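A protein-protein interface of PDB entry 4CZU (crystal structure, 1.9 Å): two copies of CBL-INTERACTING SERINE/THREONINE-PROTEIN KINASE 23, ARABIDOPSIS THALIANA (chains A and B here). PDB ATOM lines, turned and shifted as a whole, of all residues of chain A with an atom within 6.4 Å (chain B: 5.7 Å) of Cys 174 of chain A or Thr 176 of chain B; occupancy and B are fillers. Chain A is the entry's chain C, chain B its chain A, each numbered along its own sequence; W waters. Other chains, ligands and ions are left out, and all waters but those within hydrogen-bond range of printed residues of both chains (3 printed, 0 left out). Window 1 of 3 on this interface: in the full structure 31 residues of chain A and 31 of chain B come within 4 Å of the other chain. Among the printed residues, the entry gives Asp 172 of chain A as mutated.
The side-chain hydroxyl of Tyr 179 of chain B sits at hydrogen-bond distance from the side-chain carboxylate of Asp 172 of chain A (2.5 Å).
The side-chain sulfur of Cys 174 of chain B is disulfide-bonded to the side-chain sulfur of Cys 174 of chain A (2.1 Å).
The backbone carbonyl oxygen (O) of Cys 174 of chain B lies close to the backbone NH (N) of Gly 175 of chain A.
OG1 of Thr 176 of chain B sits at hydrogen-bond distance from O of Thr 173 of chain A (2.9 Å).
The side-chain carboxylate (OE1) of Glu 140 of chain A sits at hydrogen-bond distance from the side-chain hydroxyl (OG1) of Thr 173 of chain A (2.6 Å).
ND2 of Asn 178 of chain A lies close to O of Gly 175 of chain A (3.5 Å).
The backbone carbonyl oxygen (O) of Thr 173 of chain A sits at hydrogen-bond distance from the side-chain hydroxyl (OG1) of Thr 176 of chain A (3.5 Å).
Among the printed residues, pairs that only touch across the chains: Cys 174 of chain A with Leu 170 of chain B (3.9 Å), Cys 174 of chain A with Thr 176 of chain B (3.7 Å), Gly 175 of chain A with Thr 176 of chain B (3.6 Å) and Leu 212 of chain A with Thr 173 of chain B (3.4 Å).
Cys 174 of chain A touches just these residues of chain B: Leu 170, Cys 174 and Thr 176.
Thr 176 of chain B touches just these residues of chain A: Thr 173, Cys 174 and Gly 175.
Of the printed residues of chain A, Thr 173 of chain B touches Leu 212 (3.4 Å).
Of the printed residues of chain B, Leu 212 of chain A touches Thr 173 (3.4 Å).
Of the printed residues of chain A, Cys 174 of chain B touches Cys 174 (2.1 Å) and Gly 175 (3.1 Å).
Of the printed residues of chain B, Thr 173 of chain A touches Thr 176.
Of the printed residues of chain B, Gly 175 of chain A touches Cys 174 and Thr 176.
The nearest residue of chain B that does not touch Cys 174 of chain A is Glu 140 of chain B (4.3 Å).
The nearest residue of chain A that does not touch Thr 176 of chain B is Thr 176 of chain A (4.1 Å).
The nearest printed residue of chain B that does not touch Thr 173 of chain A is Cys 174 of chain B (5.5 Å).
Printed residues of chain B that touch a printed residue of chain A: Leu 170, Thr 173, Cys 174, Thr 176 and Tyr 179.
Of the 11 printed residues of chain A, 5 touch a printed residue of chain B.
Printed residues of chain A that touch a printed residue of chain B: Asp 172, Thr 173, Cys 174, Gly 175 and Leu 212.
Among the printed residues, 8 pairs touch across the chains.
Among the printed residues, no Asp or Glu carboxylate lies within 4 Å of a Lys or Arg side-chain nitrogen of the other chain.
Thr 173 of chain A touches Thr 176 of chain B, but with the chains exchanged Thr 176 of chain A does not touch Thr 173 of chain B (7.2 Å).
Cys 174 of chain A touches Thr 176 of chain B, but with the chains exchanged Thr 176 of chain A does not touch Cys 174 of chain B (4.8 Å).
Gly 175 of chain A touches Cys 174 of chain B, but with the chains exchanged Cys 174 of chain A does not touch Gly 175 of chain B (5.7 Å).
Gly 175 of chain A touches Thr 176 of chain B, but with the chains exchanged Thr 176 of chain A does not touch Gly 175 of chain B (6.1 Å).
Positions printed for both chains: 140, 173, 174, 175, 176, 177, 178 and 179.
Of the 8 pairs that touch across the chains among the printed residues, 1 has its exchanged pair printed and touching as well.
Water W1 lies within hydrogen-bond range of the backbone carbonyl oxygen (O) of Leu 212 of chain A (2.7 Å) and the side-chain hydroxyl (OG1) of Thr 173 of chain B (2.9 Å).
Water W3 lies within hydrogen-bond range of the backbone NH (N) of Thr 173 of chain A, the side-chain hydroxyl (OG1) of Thr 176 of chain A and the side-chain amide oxygen (OD1) of Asn 178 of chain B.
Water W2 lies within hydrogen-bond range of OG1 of Thr 173 of chain B and N of Leu 212 of chain A.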
ATOM      1  N   PRO A 139     -27.780  12.275   6.724  1.00  0.00           N
ATOM      2  CA  PRO A 139     -28.956  12.792   5.997  1.00  0.00           C
ATOM      3  C   PRO A 139     -29.638  11.743   5.127  1.00  0.00           C
ATOM      4  O   PRO A 139     -30.841  11.822   4.889  1.00  0.00           O
ATOM      5  CB  PRO A 139     -28.367  13.888   5.107  1.00  0.00           C
ATOM      6  CG  PRO A 139     -27.203  14.409   5.920  1.00  0.00           C
ATOM      7  CD  PRO A 139     -26.642  13.215   6.671  1.00  0.00           C
ATOM      8  N   GLU A 140     -28.885  10.760   4.653  1.00  0.00           N
ATOM      9  CA  GLU A 140     -29.455   9.762   3.764  1.00  0.00           C
ATOM     10  C   GLU A 140     -30.409   8.827   4.527  1.00  0.00           C
ATOM     11  O   GLU A 140     -31.137   8.038   3.924  1.00  0.00           O
ATOM     12  CB  GLU A 140     -28.342   9.004   3.027  1.00  0.00           C
ATOM     13  CG  GLU A 140     -27.564   9.867   2.008  1.00  0.00           C
ATOM     14  CD  GLU A 140     -26.893  11.097   2.621  1.00  0.00           C
ATOM     15  OE1 GLU A 140     -26.212  10.953   3.665  1.00  0.00           O
ATOM     16  OE2 GLU A 140     -27.056  12.206   2.051  1.00  0.00           O
ATOM     17  N   ASP A 172     -23.506   7.790  -0.408  1.00  0.00           N
ATOM     18  CA  ASP A 172     -22.640   8.919  -0.086  1.00  0.00           C
ATOM     19  C   ASP A 172     -23.391  10.057   0.574  1.00  0.00           C
ATOM     20  O   ASP A 172     -24.605  10.218   0.423  1.00  0.00           O
ATOM     21  CB  ASP A 172     -21.788   9.396  -1.271  1.00  0.00           C
ATOM     22  CG  ASP A 172     -22.601   9.617  -2.521  1.00  0.00           C
ATOM     23  OD1 ASP A 172     -23.844   9.681  -2.411  1.00  0.00           O
ATOM     24  OD2 ASP A 172     -21.997   9.721  -3.613  1.00  0.00           O
ATOM     25  N   THR A 173     -22.629  10.829   1.332  1.00  0.00           N
ATOM     26  CA  THR A 173     -23.158  11.885   2.153  1.00  0.00           C
ATOM     27  C   THR A 173     -22.333  13.094   1.790  1.00  0.00           C
ATOM     28  O   THR A 173     -21.125  12.989   1.601  1.00  0.00           O
ATOM     29  CB  THR A 173     -22.915  11.554   3.651  1.00  0.00           C
ATOM     30  OG1 THR A 173     -23.654  10.379   4.010  1.00  0.00           O
ATOM     31  CG2 THR A 173     -23.339  12.705   4.553  1.00  0.00           C
ATOM     32  N   CYS A 174     -22.980  14.246   1.686  1.00  0.00           N
ATOM     33  CA  CYS A 174     -22.249  15.483   1.546  1.00  0.00           C
ATOM     34  C   CYS A 174     -21.744  15.864   2.927  1.00  0.00           C
ATOM     35  O   CYS A 174     -22.537  16.132   3.836  1.00  0.00           O
ATOM     36  CB  CYS A 174     -23.165  16.579   0.994  1.00  0.00           C
ATOM     37  SG  CYS A 174     -22.503  18.269   1.116  1.00  0.00           S
ATOM     38  N   GLY A 175     -20.424  15.883   3.086  1.00  0.00           N
ATOM     39  CA  GLY A 175     -19.817  16.365   4.316  1.00  0.00           C
ATOM     40  C   GLY A 175     -19.804  15.351   5.447  1.00  0.00           C
ATOM     41  O   GLY A 175     -19.954  15.712   6.605  1.00  0.00           O
ATOM     42  N   THR A 176     -19.590  14.088   5.090  1.00  0.00           N
ATOM     43  CA  THR A 176     -19.552  12.952   6.021  1.00  0.00           C
ATOM     44  C   THR A 176     -19.046  13.207   7.451  1.00  0.00           C
ATOM     45  O   THR A 176     -19.766  12.909   8.398  1.00  0.00           O
ATOM     46  CB  THR A 176     -18.743  11.788   5.421  1.00  0.00           C
ATOM     47  OG1 THR A 176     -19.043  11.679   4.024  1.00  0.00           O
ATOM     48  CG2 THR A 176     -19.045  10.473   6.160  1.00  0.00           C
ATOM     49  N   PRO A 177     -17.821  13.753   7.611  1.00  0.00           N
ATOM     50  CA  PRO A 177     -17.292  13.910   8.975  1.00  0.00           C
ATOM     51  C   PRO A 177     -18.135  14.798   9.854  1.00  0.00           C
ATOM     52  O   PRO A 177     -18.078  14.627  11.070  1.00  0.00           O
ATOM     53  CB  PRO A 177     -15.936  14.591   8.759  1.00  0.00           C
ATOM     54  CG  PRO A 177     -15.588  14.306   7.348  1.00  0.00           C
ATOM     55  CD  PRO A 177     -16.866  14.261   6.602  1.00  0.00           C
ATOM     56  N   ASN A 178     -18.874  15.750   9.280  1.00  0.00           N
ATOM     57  CA  ASN A 178     -19.705  16.644  10.100  1.00  0.00           C
ATOM     58  C   ASN A 178     -20.642  15.908  11.065  1.00  0.00           C
ATOM     59  O   ASN A 178     -20.892  16.359  12.186  1.00  0.00           O
ATOM     60  CB  ASN A 178     -20.539  17.566   9.206  1.00  0.00           C
ATOM     61  CG  ASN A 178     -19.804  18.841   8.819  1.00  0.00           C
ATOM     62  OD1 ASN A 178     -20.155  19.921   9.267  1.00  0.00           O
ATOM     63  ND2 ASN A 178     -18.798  18.725   7.956  1.00  0.00           N
ATOM     64  N   TYR A 179     -21.170  14.772  10.615  1.00  0.00           N
ATOM     65  CA  TYR A 179     -22.243  14.094  11.339  1.00  0.00           C
ATOM     66  C   TYR A 179     -21.698  13.129  12.389  1.00  0.00           C
ATOM     67  O   TYR A 179     -22.465  12.537  13.157  1.00  0.00           O
ATOM     68  CB  TYR A 179     -23.157  13.348  10.340  1.00  0.00           C
ATOM     69  CG  TYR A 179     -23.810  14.309   9.361  1.00  0.00           C
ATOM     70  CD1 TYR A 179     -24.898  15.079   9.754  1.00  0.00           C
ATOM     71  CD2 TYR A 179     -23.290  14.493   8.081  1.00  0.00           C
ATOM     72  CE1 TYR A 179     -25.483  15.979   8.884  1.00  0.00           C
ATOM     73  CE2 TYR A 179     -23.867  15.409   7.204  1.00  0.00           C
ATOM     74  CZ  TYR A 179     -24.951  16.144   7.617  1.00  0.00           C
ATOM     75  OH  TYR A 179     -25.534  17.043   6.762  1.00  0.00           O
ATOM     76  N   LEU A 212     -23.085  23.113   5.754  1.00  0.00           N
ATOM     77  CA  LEU A 212     -22.481  22.364   6.849  1.00  0.00           C
ATOM     78  C   LEU A 212     -21.756  23.268   7.838  1.00  0.00           C
ATOM     79  O   LEU A 212     -21.126  24.244   7.433  1.00  0.00           O
ATOM     80  CB  LEU A 212     -21.490  21.355   6.261  1.00  0.00           C
ATOM     81  CG  LEU A 212     -22.060  20.257   5.351  1.00  0.00           C
ATOM     82  CD1 LEU A 212     -20.942  19.702   4.499  1.00  0.00           C
ATOM     83  CD2 LEU A 212     -22.699  19.132   6.159  1.00  0.00           C
ATOM     84  N   GLU B 140     -22.446  15.817  -7.221  1.00  0.00           N
ATOM     85  CA  GLU B 140     -23.107  17.116  -7.354  1.00  0.00           C
ATOM     86  C   GLU B 140     -22.650  17.933  -8.569  1.00  0.00           C
ATOM     87  O   GLU B 140     -23.315  18.894  -8.945  1.00  0.00           O
ATOM     88  CB  GLU B 140     -22.920  17.948  -6.071  1.00  0.00           C
ATOM     89  CG  GLU B 140     -23.710  17.445  -4.848  1.00  0.00           C
ATOM     90  CD  GLU B 140     -22.996  16.308  -4.097  1.00  0.00           C
ATOM     91  OE1 GLU B 140     -21.830  15.994  -4.434  1.00  0.00           O
ATOM     92  OE2 GLU B 140     -23.605  15.728  -3.162  1.00  0.00           O
ATOM     93  N   LEU B 170     -25.959  22.960  -0.718  1.00  0.00           N
ATOM     94  CA  LEU B 170     -25.378  21.632  -0.447  1.00  0.00           C
ATOM     95  C   LEU B 170     -24.522  21.019  -1.552  1.00  0.00           C
ATOM     96  O   LEU B 170     -24.772  19.890  -1.973  1.00  0.00           O
ATOM     97  CB  LEU B 170     -26.456  20.631  -0.009  1.00  0.00           C
ATOM     98  CG  LEU B 170     -26.739  20.541   1.499  1.00  0.00           C
ATOM     99  CD1 LEU B 170     -27.613  19.332   1.805  1.00  0.00           C
ATOM    100  CD2 LEU B 170     -25.455  20.484   2.315  1.00  0.00           C
ATOM    101  N   HIS B 171     -23.501  21.745  -2.010  1.00  0.00           N
ATOM    102  CA  HIS B 171     -22.528  21.155  -2.933  1.00  0.00           C
ATOM    103  C   HIS B 171     -21.084  21.646  -2.749  1.00  0.00           C
ATOM    104  O   HIS B 171     -20.145  20.872  -2.908  1.00  0.00           O
ATOM    105  CB  HIS B 171     -22.973  21.279  -4.403  1.00  0.00           C
ATOM    106  CG  HIS B 171     -23.249  22.684  -4.836  1.00  0.00           C
ATOM    107  ND1 HIS B 171     -22.270  23.514  -5.347  1.00  0.00           N
ATOM    108  CD2 HIS B 171     -24.391  23.414  -4.818  1.00  0.00           C
ATOM    109  CE1 HIS B 171     -22.799  24.693  -5.630  1.00  0.00           C
ATOM    110  NE2 HIS B 171     -24.083  24.660  -5.315  1.00  0.00           N
ATOM    111  N   THR B 173     -19.102  22.883  -0.093  1.00  0.00           N
ATOM    112  CA  THR B 173     -18.254  22.474   1.026  1.00  0.00           C
ATOM    113  C   THR B 173     -18.492  21.032   1.451  1.00  0.00           C
ATOM    114  O   THR B 173     -18.270  20.677   2.613  1.00  0.00           O
ATOM    115  CB  THR B 173     -18.431  23.402   2.229  1.00  0.00           C
ATOM    116  OG1 THR B 173     -19.821  23.453   2.589  1.00  0.00           O
ATOM    117  CG2 THR B 173     -17.938  24.822   1.885  1.00  0.00           C
ATOM    118  N   CYS B 174     -18.935  20.211   0.505  1.00  0.00           N
ATOM    119  CA  CYS B 174     -19.154  18.794   0.751  1.00  0.00           C
ATOM    120  C   CYS B 174     -17.866  18.081   1.149  1.00  0.00           C
ATOM    121  O   CYS B 174     -17.829  17.412   2.180  1.00  0.00           O
ATOM    122  CB  CYS B 174     -19.791  18.125  -0.471  1.00  0.00           C
ATOM    123  SG  CYS B 174     -21.545  18.567  -0.676  1.00  0.00           S
ATOM    124  N   GLY B 175     -16.818  18.217   0.336  1.00  0.00           N
ATOM    125  CA  GLY B 175     -15.525  17.636   0.671  1.00  0.00           C
ATOM    126  C   GLY B 175     -15.551  16.140   0.962  1.00  0.00           C
ATOM    127  O   GLY B 175     -14.761  15.634   1.761  1.00  0.00           O
ATOM    128  N   THR B 176     -16.450  15.423   0.292  1.00  0.00           N
ATOM    129  CA  THR B 176     -16.612  13.983   0.503  1.00  0.00           C
ATOM    130  C   THR B 176     -15.379  13.172   0.071  1.00  0.00           C
ATOM    131  O   THR B 176     -15.020  13.160  -1.109  1.00  0.00           O
ATOM    132  CB  THR B 176     -17.876  13.485  -0.243  1.00  0.00           C
ATOM    133  OG1 THR B 176     -19.008  14.263   0.177  1.00  0.00           O
ATOM    134  CG2 THR B 176     -18.138  12.012   0.023  1.00  0.00           C
ATOM    135  N   PRO B 177     -14.746  12.459   1.022  1.00  0.00           N
ATOM    136  CA  PRO B 177     -13.483  11.749   0.781  1.00  0.00           C
ATOM    137  C   PRO B 177     -13.558  10.585  -0.205  1.00  0.00           C
ATOM    138  O   PRO B 177     -12.534  10.215  -0.780  1.00  0.00           O
ATOM    139  CB  PRO B 177     -13.107  11.221   2.168  1.00  0.00           C
ATOM    140  CG  PRO B 177     -14.367  11.166   2.895  1.00  0.00           C
ATOM    141  CD  PRO B 177     -15.170  12.331   2.423  1.00  0.00           C
ATOM    142  N   ASN B 178     -14.746  10.028  -0.401  1.00  0.00           N
ATOM    143  CA  ASN B 178     -14.912   8.846  -1.247  1.00  0.00           C
ATOM    144  C   ASN B 178     -14.505   9.074  -2.699  1.00  0.00           C
ATOM    145  O   ASN B 178     -14.137   8.123  -3.394  1.00  0.00           O
ATOM    146  CB  ASN B 178     -16.361   8.332  -1.170  1.00  0.00           C
ATOM    147  CG  ASN B 178     -16.846   8.180   0.257  1.00  0.00           C
ATOM    148  OD1 ASN B 178     -17.108   9.170   0.940  1.00  0.00           O
ATOM    149  ND2 ASN B 178     -16.984   6.928   0.720  1.00  0.00           N
ATOM    150  N   TYR B 179     -14.554  10.335  -3.135  1.00  0.00           N
ATOM    151  CA  TYR B 179     -14.231  10.718  -4.513  1.00  0.00           C
ATOM    152  C   TYR B 179     -12.808  11.274  -4.668  1.00  0.00           C
ATOM    153  O   TYR B 179     -12.368  11.575  -5.783  1.00  0.00           O
ATOM    154  CB  TYR B 179     -15.275  11.736  -5.012  1.00  0.00           C
ATOM    155  CG  TYR B 179     -16.629  11.077  -5.082  1.00  0.00           C
ATOM    156  CD1 TYR B 179     -16.952  10.266  -6.161  1.00  0.00           C
ATOM    157  CD2 TYR B 179     -17.542  11.188  -4.034  1.00  0.00           C
ATOM    158  CE1 TYR B 179     -18.180   9.603  -6.227  1.00  0.00           C
ATOM    159  CE2 TYR B 179     -18.772  10.521  -4.084  1.00  0.00           C
ATOM    160  CZ  TYR B 179     -19.078   9.736  -5.187  1.00  0.00           C
ATOM    161  OH  TYR B 179     -20.293   9.080  -5.270  1.00  0.00           O
ATOM    162  N   VAL B 180     -12.096  11.382  -3.555  1.00  0.00           N
ATOM    163  CA  VAL B 180     -10.820  12.097  -3.519  1.00  0.00           C
ATOM    164  C   VAL B 180      -9.610  11.157  -3.571  1.00  0.00           C
ATOM    165  O   VAL B 180      -9.595  10.120  -2.897  1.00  0.00           O
ATOM    166  CB  VAL B 180     -10.734  12.964  -2.234  1.00  0.00           C
ATOM    167  CG1 VAL B 180      -9.482  13.837  -2.255  1.00  0.00           C
ATOM    168  CG2 VAL B 180     -11.995  13.833  -2.077  1.00  0.00           C
HETATM  169  O   HOH W   1     -20.320  25.059   4.973  1.00  0.00           O
HETATM  170  O   HOH W   2     -22.525  22.658   2.871  1.00  0.00           O
HETATM  171  O   HOH W   3     -20.247   9.640   2.020  1.00  0.00           O
